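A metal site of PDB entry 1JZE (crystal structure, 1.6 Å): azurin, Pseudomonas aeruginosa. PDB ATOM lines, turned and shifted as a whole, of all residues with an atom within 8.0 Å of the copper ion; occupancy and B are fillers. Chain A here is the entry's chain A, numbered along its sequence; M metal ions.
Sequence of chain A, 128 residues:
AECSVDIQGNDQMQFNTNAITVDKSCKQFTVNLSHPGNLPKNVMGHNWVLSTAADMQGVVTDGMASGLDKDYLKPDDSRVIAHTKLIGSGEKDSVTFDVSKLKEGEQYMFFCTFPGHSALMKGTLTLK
A ring nitrogen (ND1) of His 117 sits close to the backbone carbonyl oxygen (O) of Gly 45, 3.2 Å away. A ring nitrogen (ND1) of His 117 lies close to the side-chain sulfur of Met 121. A ring nitrogen (NE2) of His 46 is in hydrogen-bond range of the backbone carbonyl oxygen (O) of Asn 10, at 2.6 Å. OD1 of Asn 47 sits close to SG of Cys 112 (3.6 Å). The side-chain sulfur (SG) of Cys 112 lies close to the backbone carbonyl oxygen (O) of Gly 45 (3.6 Å). O of Met 121 sits at hydrogen-bond distance from N of Cys 112, 3.2 Å away. NE2 of His 117 lies close to SD of Met 44 (3.8 Å). A ring nitrogen (ND1) of His 46 sits close to the side-chain sulfur (SD) of Met 121, 3.0 Å away.
CB of Phe 114 touches the copper ion, at 3.9 Å. Met 121 touches the copper ion (SD to CU, 3.1 Å). Within 4 Å of the copper ion: Gly 45, His 46, Cys 112, Phe 114, His 117 and Met 121.
The copper ion is bound by a ring nitrogen (ND1) of His 46 (2.0 Å), a ring nitrogen (ND1) of His 117 (2.0 Å) and the side-chain sulfur of Cys 112 (2.2 Å). Slightly farther from the copper ion lies O of Gly 45 (2.7 Å).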
ATOM      1  N   GLY A   9     -28.546 -31.719  19.657  1.00  0.00           N
ATOM      2  CA  GLY A   9     -29.338 -30.711  20.346  1.00  0.00           C
ATOM      3  C   GLY A   9     -30.029 -29.934  19.242  1.00  0.00           C
ATOM      4  O   GLY A   9     -29.360 -29.422  18.345  1.00  0.00           O
ATOM      5  N   ASN A  10     -31.346 -29.767  19.324  1.00  0.00           N
ATOM      6  CA  ASN A  10     -32.081 -29.067  18.269  1.00  0.00           C
ATOM      7  C   ASN A  10     -32.709 -27.707  18.568  1.00  0.00           C
ATOM      8  O   ASN A  10     -32.474 -27.108  19.624  1.00  0.00           O
ATOM      9  CB  ASN A  10     -33.183 -29.994  17.717  1.00  0.00           C
ATOM     10  CG  ASN A  10     -34.326 -30.177  18.695  1.00  0.00           C
ATOM     11  OD1 ASN A  10     -34.405 -29.492  19.710  1.00  0.00           O
ATOM     12  ND2 ASN A  10     -35.220 -31.086  18.380  1.00  0.00           N
ATOM     13  N   MET A  13     -35.288 -27.345  21.540  1.00  0.00           N
ATOM     14  CA  MET A  13     -34.671 -27.521  22.845  1.00  0.00           C
ATOM     15  C   MET A  13     -34.713 -28.977  23.239  1.00  0.00           C
ATOM     16  O   MET A  13     -35.126 -29.305  24.348  1.00  0.00           O
ATOM     17  CB  MET A  13     -35.445 -26.740  23.913  1.00  0.00           C
ATOM     18  CG  MET A  13     -34.998 -25.331  24.171  1.00  0.00           C
ATOM     19  SD  MET A  13     -35.755 -24.707  25.683  1.00  0.00           S
ATOM     20  CE  MET A  13     -37.209 -25.814  25.849  1.00  0.00           C
ATOM     21  N   GLN A  14     -34.328 -29.866  22.342  1.00  0.00           N
ATOM     22  CA  GLN A  14     -34.357 -31.270  22.669  1.00  0.00           C
ATOM     23  C   GLN A  14     -33.055 -31.979  22.339  1.00  0.00           C
ATOM     24  O   GLN A  14     -32.371 -31.644  21.374  1.00  0.00           O
ATOM     25  CB  GLN A  14     -35.510 -31.945  21.913  1.00  0.00           C
ATOM     26  CG  GLN A  14     -36.884 -31.593  22.452  1.00  0.00           C
ATOM     27  CD  GLN A  14     -38.005 -32.024  21.527  1.00  0.00           C
ATOM     28  OE1 GLN A  14     -39.067 -32.462  21.991  1.00  0.00           O
ATOM     29  NE2 GLN A  14     -37.782 -31.892  20.229  1.00  0.00           N
ATOM     30  N   PHE A  15     -32.681 -32.885  23.253  1.00  0.00           N
ATOM     31  CA  PHE A  15     -31.526 -33.756  23.083  1.00  0.00           C
ATOM     32  C   PHE A  15     -32.212 -34.993  22.516  1.00  0.00           C
ATOM     33  O   PHE A  15     -33.380 -35.258  22.834  1.00  0.00           O
ATOM     34  CB  PHE A  15     -30.916 -34.174  24.432  1.00  0.00           C
ATOM     35  CG  PHE A  15     -29.879 -33.235  24.961  1.00  0.00           C
ATOM     36  CD1 PHE A  15     -28.975 -32.605  24.098  1.00  0.00           C
ATOM     37  CD2 PHE A  15     -29.761 -33.020  26.324  1.00  0.00           C
ATOM     38  CE1 PHE A  15     -27.976 -31.768  24.602  1.00  0.00           C
ATOM     39  CE2 PHE A  15     -28.768 -32.176  26.834  1.00  0.00           C
ATOM     40  CZ  PHE A  15     -27.877 -31.559  25.953  1.00  0.00           C
ATOM     41  N   LEU A  33     -21.298 -34.103  20.627  1.00  0.00           N
ATOM     42  CA  LEU A  33     -22.468 -33.247  20.505  1.00  0.00           C
ATOM     43  C   LEU A  33     -22.531 -32.477  19.195  1.00  0.00           C
ATOM     44  O   LEU A  33     -21.544 -31.885  18.768  1.00  0.00           O
ATOM     45  CB  LEU A  33     -22.514 -32.255  21.662  1.00  0.00           C
ATOM     46  CG  LEU A  33     -23.647 -31.223  21.605  1.00  0.00           C
ATOM     47  CD1 LEU A  33     -24.979 -31.898  21.925  1.00  0.00           C
ATOM     48  CD2 LEU A  33     -23.357 -30.077  22.576  1.00  0.00           C
ATOM     49  N   HIS A  35     -25.307 -29.946  16.522  1.00  0.00           N
ATOM     50  CA  HIS A  35     -26.482 -29.082  16.497  1.00  0.00           C
ATOM     51  C   HIS A  35     -27.101 -29.037  15.107  1.00  0.00           C
ATOM     52  O   HIS A  35     -26.691 -28.239  14.261  1.00  0.00           O
ATOM     53  CB  HIS A  35     -26.050 -27.679  16.949  1.00  0.00           C
ATOM     54  CG  HIS A  35     -27.166 -26.777  17.339  1.00  0.00           C
ATOM     55  ND1 HIS A  35     -28.290 -26.583  16.547  1.00  0.00           N
ATOM     56  CD2 HIS A  35     -27.320 -25.969  18.411  1.00  0.00           C
ATOM     57  CE1 HIS A  35     -29.068 -25.688  17.128  1.00  0.00           C
ATOM     58  NE2 HIS A  35     -28.513 -25.300  18.251  1.00  0.00           N
ATOM     59  N   LYS A  41     -26.081 -19.940  18.494  1.00  0.00           N
ATOM     60  CA  LYS A  41     -25.940 -20.296  19.901  1.00  0.00           C
ATOM     61  C   LYS A  41     -26.386 -19.254  20.886  1.00  0.00           C
ATOM     62  O   LYS A  41     -26.550 -19.577  22.066  1.00  0.00           O
ATOM     63  CB  LYS A  41     -24.535 -20.767  20.232  1.00  0.00           C
ATOM     64  CG  LYS A  41     -23.473 -19.710  20.185  1.00  0.00           C
ATOM     65  CD  LYS A  41     -22.132 -20.352  20.475  1.00  0.00           C
ATOM     66  CE  LYS A  41     -21.045 -19.303  20.537  1.00  0.00           C
ATOM     67  NZ  LYS A  41     -19.710 -19.917  20.732  1.00  0.00           N
ATOM     68  N   VAL A  43     -29.268 -17.793  20.801  1.00  0.00           N
ATOM     69  CA  VAL A  43     -30.710 -17.948  20.997  1.00  0.00           C
ATOM     70  C   VAL A  43     -31.067 -19.393  21.274  1.00  0.00           C
ATOM     71  O   VAL A  43     -31.992 -19.667  22.004  1.00  0.00           O
ATOM     72  CB  VAL A  43     -31.575 -17.449  19.781  1.00  0.00           C
ATOM     73  CG1 VAL A  43     -31.041 -16.163  19.188  1.00  0.00           C
ATOM     74  CG2 VAL A  43     -31.726 -18.543  18.718  1.00  0.00           C
ATOM     75  N   MET A  44     -30.287 -20.328  20.724  1.00  0.00           N
ATOM     76  CA  MET A  44     -30.564 -21.747  20.900  1.00  0.00           C
ATOM     77  C   MET A  44     -29.282 -22.535  21.123  1.00  0.00           C
ATOM     78  O   MET A  44     -29.116 -23.639  20.619  1.00  0.00           O
ATOM     79  CB  MET A  44     -31.286 -22.263  19.658  1.00  0.00           C
ATOM     80  CG  MET A  44     -31.892 -23.664  19.768  1.00  0.00           C
ATOM     81  SD  MET A  44     -32.881 -23.904  21.223  1.00  0.00           S
ATOM     82  CE  MET A  44     -34.352 -22.982  20.748  1.00  0.00           C
ATOM     83  N   GLY A  45     -28.373 -21.948  21.894  1.00  0.00           N
ATOM     84  CA  GLY A  45     -27.109 -22.612  22.153  1.00  0.00           C
ATOM     85  C   GLY A  45     -27.271 -23.860  23.007  1.00  0.00           C
ATOM     86  O   GLY A  45     -28.125 -23.921  23.884  1.00  0.00           O
ATOM     87  N   HIS A  46     -26.451 -24.864  22.726  1.00  0.00           N
ATOM     88  CA  HIS A  46     -26.499 -26.100  23.475  1.00  0.00           C
ATOM     89  C   HIS A  46     -25.140 -26.603  23.892  1.00  0.00           C
ATOM     90  O   HIS A  46     -24.169 -26.591  23.132  1.00  0.00           O
ATOM     91  CB  HIS A  46     -27.164 -27.226  22.687  1.00  0.00           C
ATOM     92  CG  HIS A  46     -28.582 -26.960  22.294  1.00  0.00           C
ATOM     93  ND1 HIS A  46     -29.549 -26.533  23.175  1.00  0.00           N
ATOM     94  CD2 HIS A  46     -29.208 -27.091  21.089  1.00  0.00           C
ATOM     95  CE1 HIS A  46     -30.704 -26.417  22.539  1.00  0.00           C
ATOM     96  NE2 HIS A  46     -30.515 -26.749  21.283  1.00  0.00           N
ATOM     97  N   ASN A  47     -25.072 -27.076  25.129  1.00  0.00           N
ATOM     98  CA  ASN A  47     -23.862 -27.697  25.596  1.00  0.00           C
ATOM     99  C   ASN A  47     -24.301 -28.961  26.310  1.00  0.00           C
ATOM    100  O   ASN A  47     -25.498 -29.191  26.541  1.00  0.00           O
ATOM    101  CB  ASN A  47     -23.023 -26.788  26.519  1.00  0.00           C
ATOM    102  CG  ASN A  47     -23.792 -26.260  27.711  1.00  0.00           C
ATOM    103  OD1 ASN A  47     -24.894 -26.698  28.025  1.00  0.00           O
ATOM    104  ND2 ASN A  47     -23.183 -25.306  28.413  1.00  0.00           N
ATOM    105  N   TRP A  48     -23.336 -29.830  26.559  1.00  0.00           N
ATOM    106  CA  TRP A  48     -23.614 -31.074  27.261  1.00  0.00           C
ATOM    107  C   TRP A  48     -22.759 -30.976  28.507  1.00  0.00           C
ATOM    108  O   TRP A  48     -21.544 -30.975  28.420  1.00  0.00           O
ATOM    109  CB  TRP A  48     -23.202 -32.261  26.398  1.00  0.00           C
ATOM    110  CG  TRP A  48     -23.575 -33.588  26.995  1.00  0.00           C
ATOM    111  CD1 TRP A  48     -24.728 -34.282  26.812  1.00  0.00           C
ATOM    112  CD2 TRP A  48     -22.755 -34.403  27.883  1.00  0.00           C
ATOM    113  NE1 TRP A  48     -24.692 -35.470  27.512  1.00  0.00           N
ATOM    114  CE2 TRP A  48     -23.488 -35.555  28.178  1.00  0.00           C
ATOM    115  CE3 TRP A  48     -21.486 -34.238  28.444  1.00  0.00           C
ATOM    116  CZ2 TRP A  48     -23.011 -36.569  29.027  1.00  0.00           C
ATOM    117  CZ3 TRP A  48     -20.990 -35.253  29.291  1.00  0.00           C
ATOM    118  CH2 TRP A  48     -21.749 -36.400  29.556  1.00  0.00           C
ATOM    119  N   LEU A  86     -20.489 -24.436  24.414  1.00  0.00           N
ATOM    120  CA  LEU A  86     -21.815 -24.124  23.926  1.00  0.00           C
ATOM    121  C   LEU A  86     -21.725 -24.021  22.405  1.00  0.00           C
ATOM    122  O   LEU A  86     -20.824 -23.363  21.889  1.00  0.00           O
ATOM    123  CB  LEU A  86     -22.302 -22.785  24.498  1.00  0.00           C
ATOM    124  CG  LEU A  86     -23.799 -22.512  24.314  1.00  0.00           C
ATOM    125  CD1 LEU A  86     -24.569 -23.267  25.386  1.00  0.00           C
ATOM    126  CD2 LEU A  86     -24.085 -21.027  24.430  1.00  0.00           C
ATOM    127  N   ILE A  87     -22.636 -24.681  21.701  1.00  0.00           N
ATOM    128  CA  ILE A  87     -22.647 -24.649  20.238  1.00  0.00           C
ATOM    129  C   ILE A  87     -23.981 -24.217  19.620  1.00  0.00           C
ATOM    130  O   ILE A  87     -25.040 -24.368  20.220  1.00  0.00           O
ATOM    131  CB  ILE A  87     -22.266 -26.024  19.644  1.00  0.00           C
ATOM    132  CG1 ILE A  87     -23.284 -27.088  20.071  1.00  0.00           C
ATOM    133  CG2 ILE A  87     -20.869 -26.425  20.085  1.00  0.00           C
ATOM    134  CD1 ILE A  87     -23.082 -28.423  19.382  1.00  0.00           C
ATOM    135  N   PHE A 111     -26.968 -32.258  31.086  1.00  0.00           N
ATOM    136  CA  PHE A 111     -27.919 -31.218  30.737  1.00  0.00           C
ATOM    137  C   PHE A 111     -27.238 -30.063  30.039  1.00  0.00           C
ATOM    138  O   PHE A 111     -26.004 -29.965  30.019  1.00  0.00           O
ATOM    139  CB  PHE A 111     -28.572 -30.707  32.026  1.00  0.00           C
ATOM    140  CG  PHE A 111     -27.591 -30.435  33.132  1.00  0.00           C
ATOM    141  CD1 PHE A 111     -27.232 -31.446  34.026  1.00  0.00           C
ATOM    142  CD2 PHE A 111     -26.945 -29.209  33.233  1.00  0.00           C
ATOM    143  CE1 PHE A 111     -26.257 -31.247  34.993  1.00  0.00           C
ATOM    144  CE2 PHE A 111     -25.969 -28.996  34.202  1.00  0.00           C
ATOM    145  CZ  PHE A 111     -25.622 -30.013  35.093  1.00  0.00           C
ATOM    146  N   CYS A 112     -28.073 -29.190  29.488  1.00  0.00           N
ATOM    147  CA  CYS A 112     -27.650 -27.981  28.805  1.00  0.00           C
ATOM    148  C   CYS A 112     -27.862 -26.846  29.795  1.00  0.00           C
ATOM    149  O   CYS A 112     -28.916 -26.750  30.419  1.00  0.00           O
ATOM    150  CB  CYS A 112     -28.531 -27.725  27.587  1.00  0.00           C
ATOM    151  SG  CYS A 112     -28.156 -26.174  26.725  1.00  0.00           S
ATOM    152  N   THR A 113     -26.891 -25.943  29.902  1.00  0.00           N
ATOM    153  CA  THR A 113     -27.021 -24.836  30.821  1.00  0.00           C
ATOM    154  C   THR A 113     -27.524 -23.534  30.210  1.00  0.00           C
ATOM    155  O   THR A 113     -27.575 -22.516  30.891  1.00  0.00           O
ATOM    156  CB  THR A 113     -25.718 -24.552  31.583  1.00  0.00           C
ATOM    157  OG1 THR A 113     -24.639 -24.334  30.664  1.00  0.00           O
ATOM    158  CG2 THR A 113     -25.394 -25.737  32.505  1.00  0.00           C
ATOM    159  N   PHE A 114     -27.865 -23.546  28.921  1.00  0.00           N
ATOM    160  CA  PHE A 114     -28.377 -22.332  28.277  1.00  0.00           C
ATOM    161  C   PHE A 114     -29.716 -22.043  28.998  1.00  0.00           C
ATOM    162  O   PHE A 114     -30.515 -22.945  29.207  1.00  0.00           O
ATOM    163  CB  PHE A 114     -28.602 -22.576  26.789  1.00  0.00           C
ATOM    164  CG  PHE A 114     -29.013 -21.348  26.025  1.00  0.00           C
ATOM    165  CD1 PHE A 114     -30.335 -20.895  26.053  1.00  0.00           C
ATOM    166  CD2 PHE A 114     -28.068 -20.618  25.301  1.00  0.00           C
ATOM    167  CE1 PHE A 114     -30.699 -19.738  25.383  1.00  0.00           C
ATOM    168  CE2 PHE A 114     -28.439 -19.460  24.623  1.00  0.00           C
ATOM    169  CZ  PHE A 114     -29.754 -19.017  24.671  1.00  0.00           C
ATOM    170  N   PRO A 115     -29.946 -20.785  29.384  1.00  0.00           N
ATOM    171  CA  PRO A 115     -31.157 -20.361  30.087  1.00  0.00           C
ATOM    172  C   PRO A 115     -32.470 -21.047  29.684  1.00  0.00           C
ATOM    173  O   PRO A 115     -32.887 -20.983  28.523  1.00  0.00           O
ATOM    174  CB  PRO A 115     -31.187 -18.863  29.812  1.00  0.00           C
ATOM    175  CG  PRO A 115     -29.712 -18.537  29.957  1.00  0.00           C
ATOM    176  CD  PRO A 115     -29.078 -19.632  29.108  1.00  0.00           C
ATOM    177  N   GLY A 116     -33.051 -21.762  30.633  1.00  0.00           N
ATOM    178  CA  GLY A 116     -34.309 -22.458  30.444  1.00  0.00           C
ATOM    179  C   GLY A 116     -34.270 -23.818  29.755  1.00  0.00           C
ATOM    180  O   GLY A 116     -35.224 -24.581  29.866  1.00  0.00           O
ATOM    181  N   HIS A 117     -33.165 -24.145  29.090  1.00  0.00           N
ATOM    182  CA  HIS A 117     -33.080 -25.402  28.379  1.00  0.00           C
ATOM    183  C   HIS A 117     -33.132 -26.653  29.234  1.00  0.00           C
ATOM    184  O   HIS A 117     -33.838 -27.599  28.888  1.00  0.00           O
ATOM    185  CB  HIS A 117     -31.828 -25.453  27.509  1.00  0.00           C
ATOM    186  CG  HIS A 117     -31.869 -24.538  26.322  1.00  0.00           C
ATOM    187  ND1 HIS A 117     -30.966 -24.641  25.285  1.00  0.00           N
ATOM    188  CD2 HIS A 117     -32.671 -23.502  26.032  1.00  0.00           C
ATOM    189  CE1 HIS A 117     -31.210 -23.685  24.403  1.00  0.00           C
ATOM    190  NE2 HIS A 117     -32.256 -22.977  24.835  1.00  0.00           N
ATOM    191  N   SER A 118     -32.410 -26.648  30.351  1.00  0.00           N
ATOM    192  CA  SER A 118     -32.343 -27.800  31.241  1.00  0.00           C
ATOM    193  C   SER A 118     -33.683 -28.382  31.662  1.00  0.00           C
ATOM    194  O   SER A 118     -33.744 -29.526  32.124  1.00  0.00           O
ATOM    195  CB  SER A 118     -31.469 -27.499  32.466  1.00  0.00           C
ATOM    196  OG  SER A 118     -32.190 -26.856  33.494  1.00  0.00           O
ATOM    197  N   MET A 121     -34.043 -30.161  28.057  1.00  0.00           N
ATOM    198  CA  MET A 121     -32.738 -30.722  27.736  1.00  0.00           C
ATOM    199  C   MET A 121     -31.902 -31.273  28.876  1.00  0.00           C
ATOM    200  O   MET A 121     -30.902 -30.679  29.287  1.00  0.00           O
ATOM    201  CB  MET A 121     -31.908 -29.703  26.960  1.00  0.00           C
ATOM    202  CG  MET A 121     -32.616 -29.182  25.761  1.00  0.00           C
ATOM    203  SD  MET A 121     -31.580 -28.202  24.717  1.00  0.00           S
ATOM    204  CE  MET A 121     -30.276 -29.370  24.349  1.00  0.00           C
HETATM  205 CU    CU M   1     -29.477 -25.901  25.024  1.00  0.00          CU
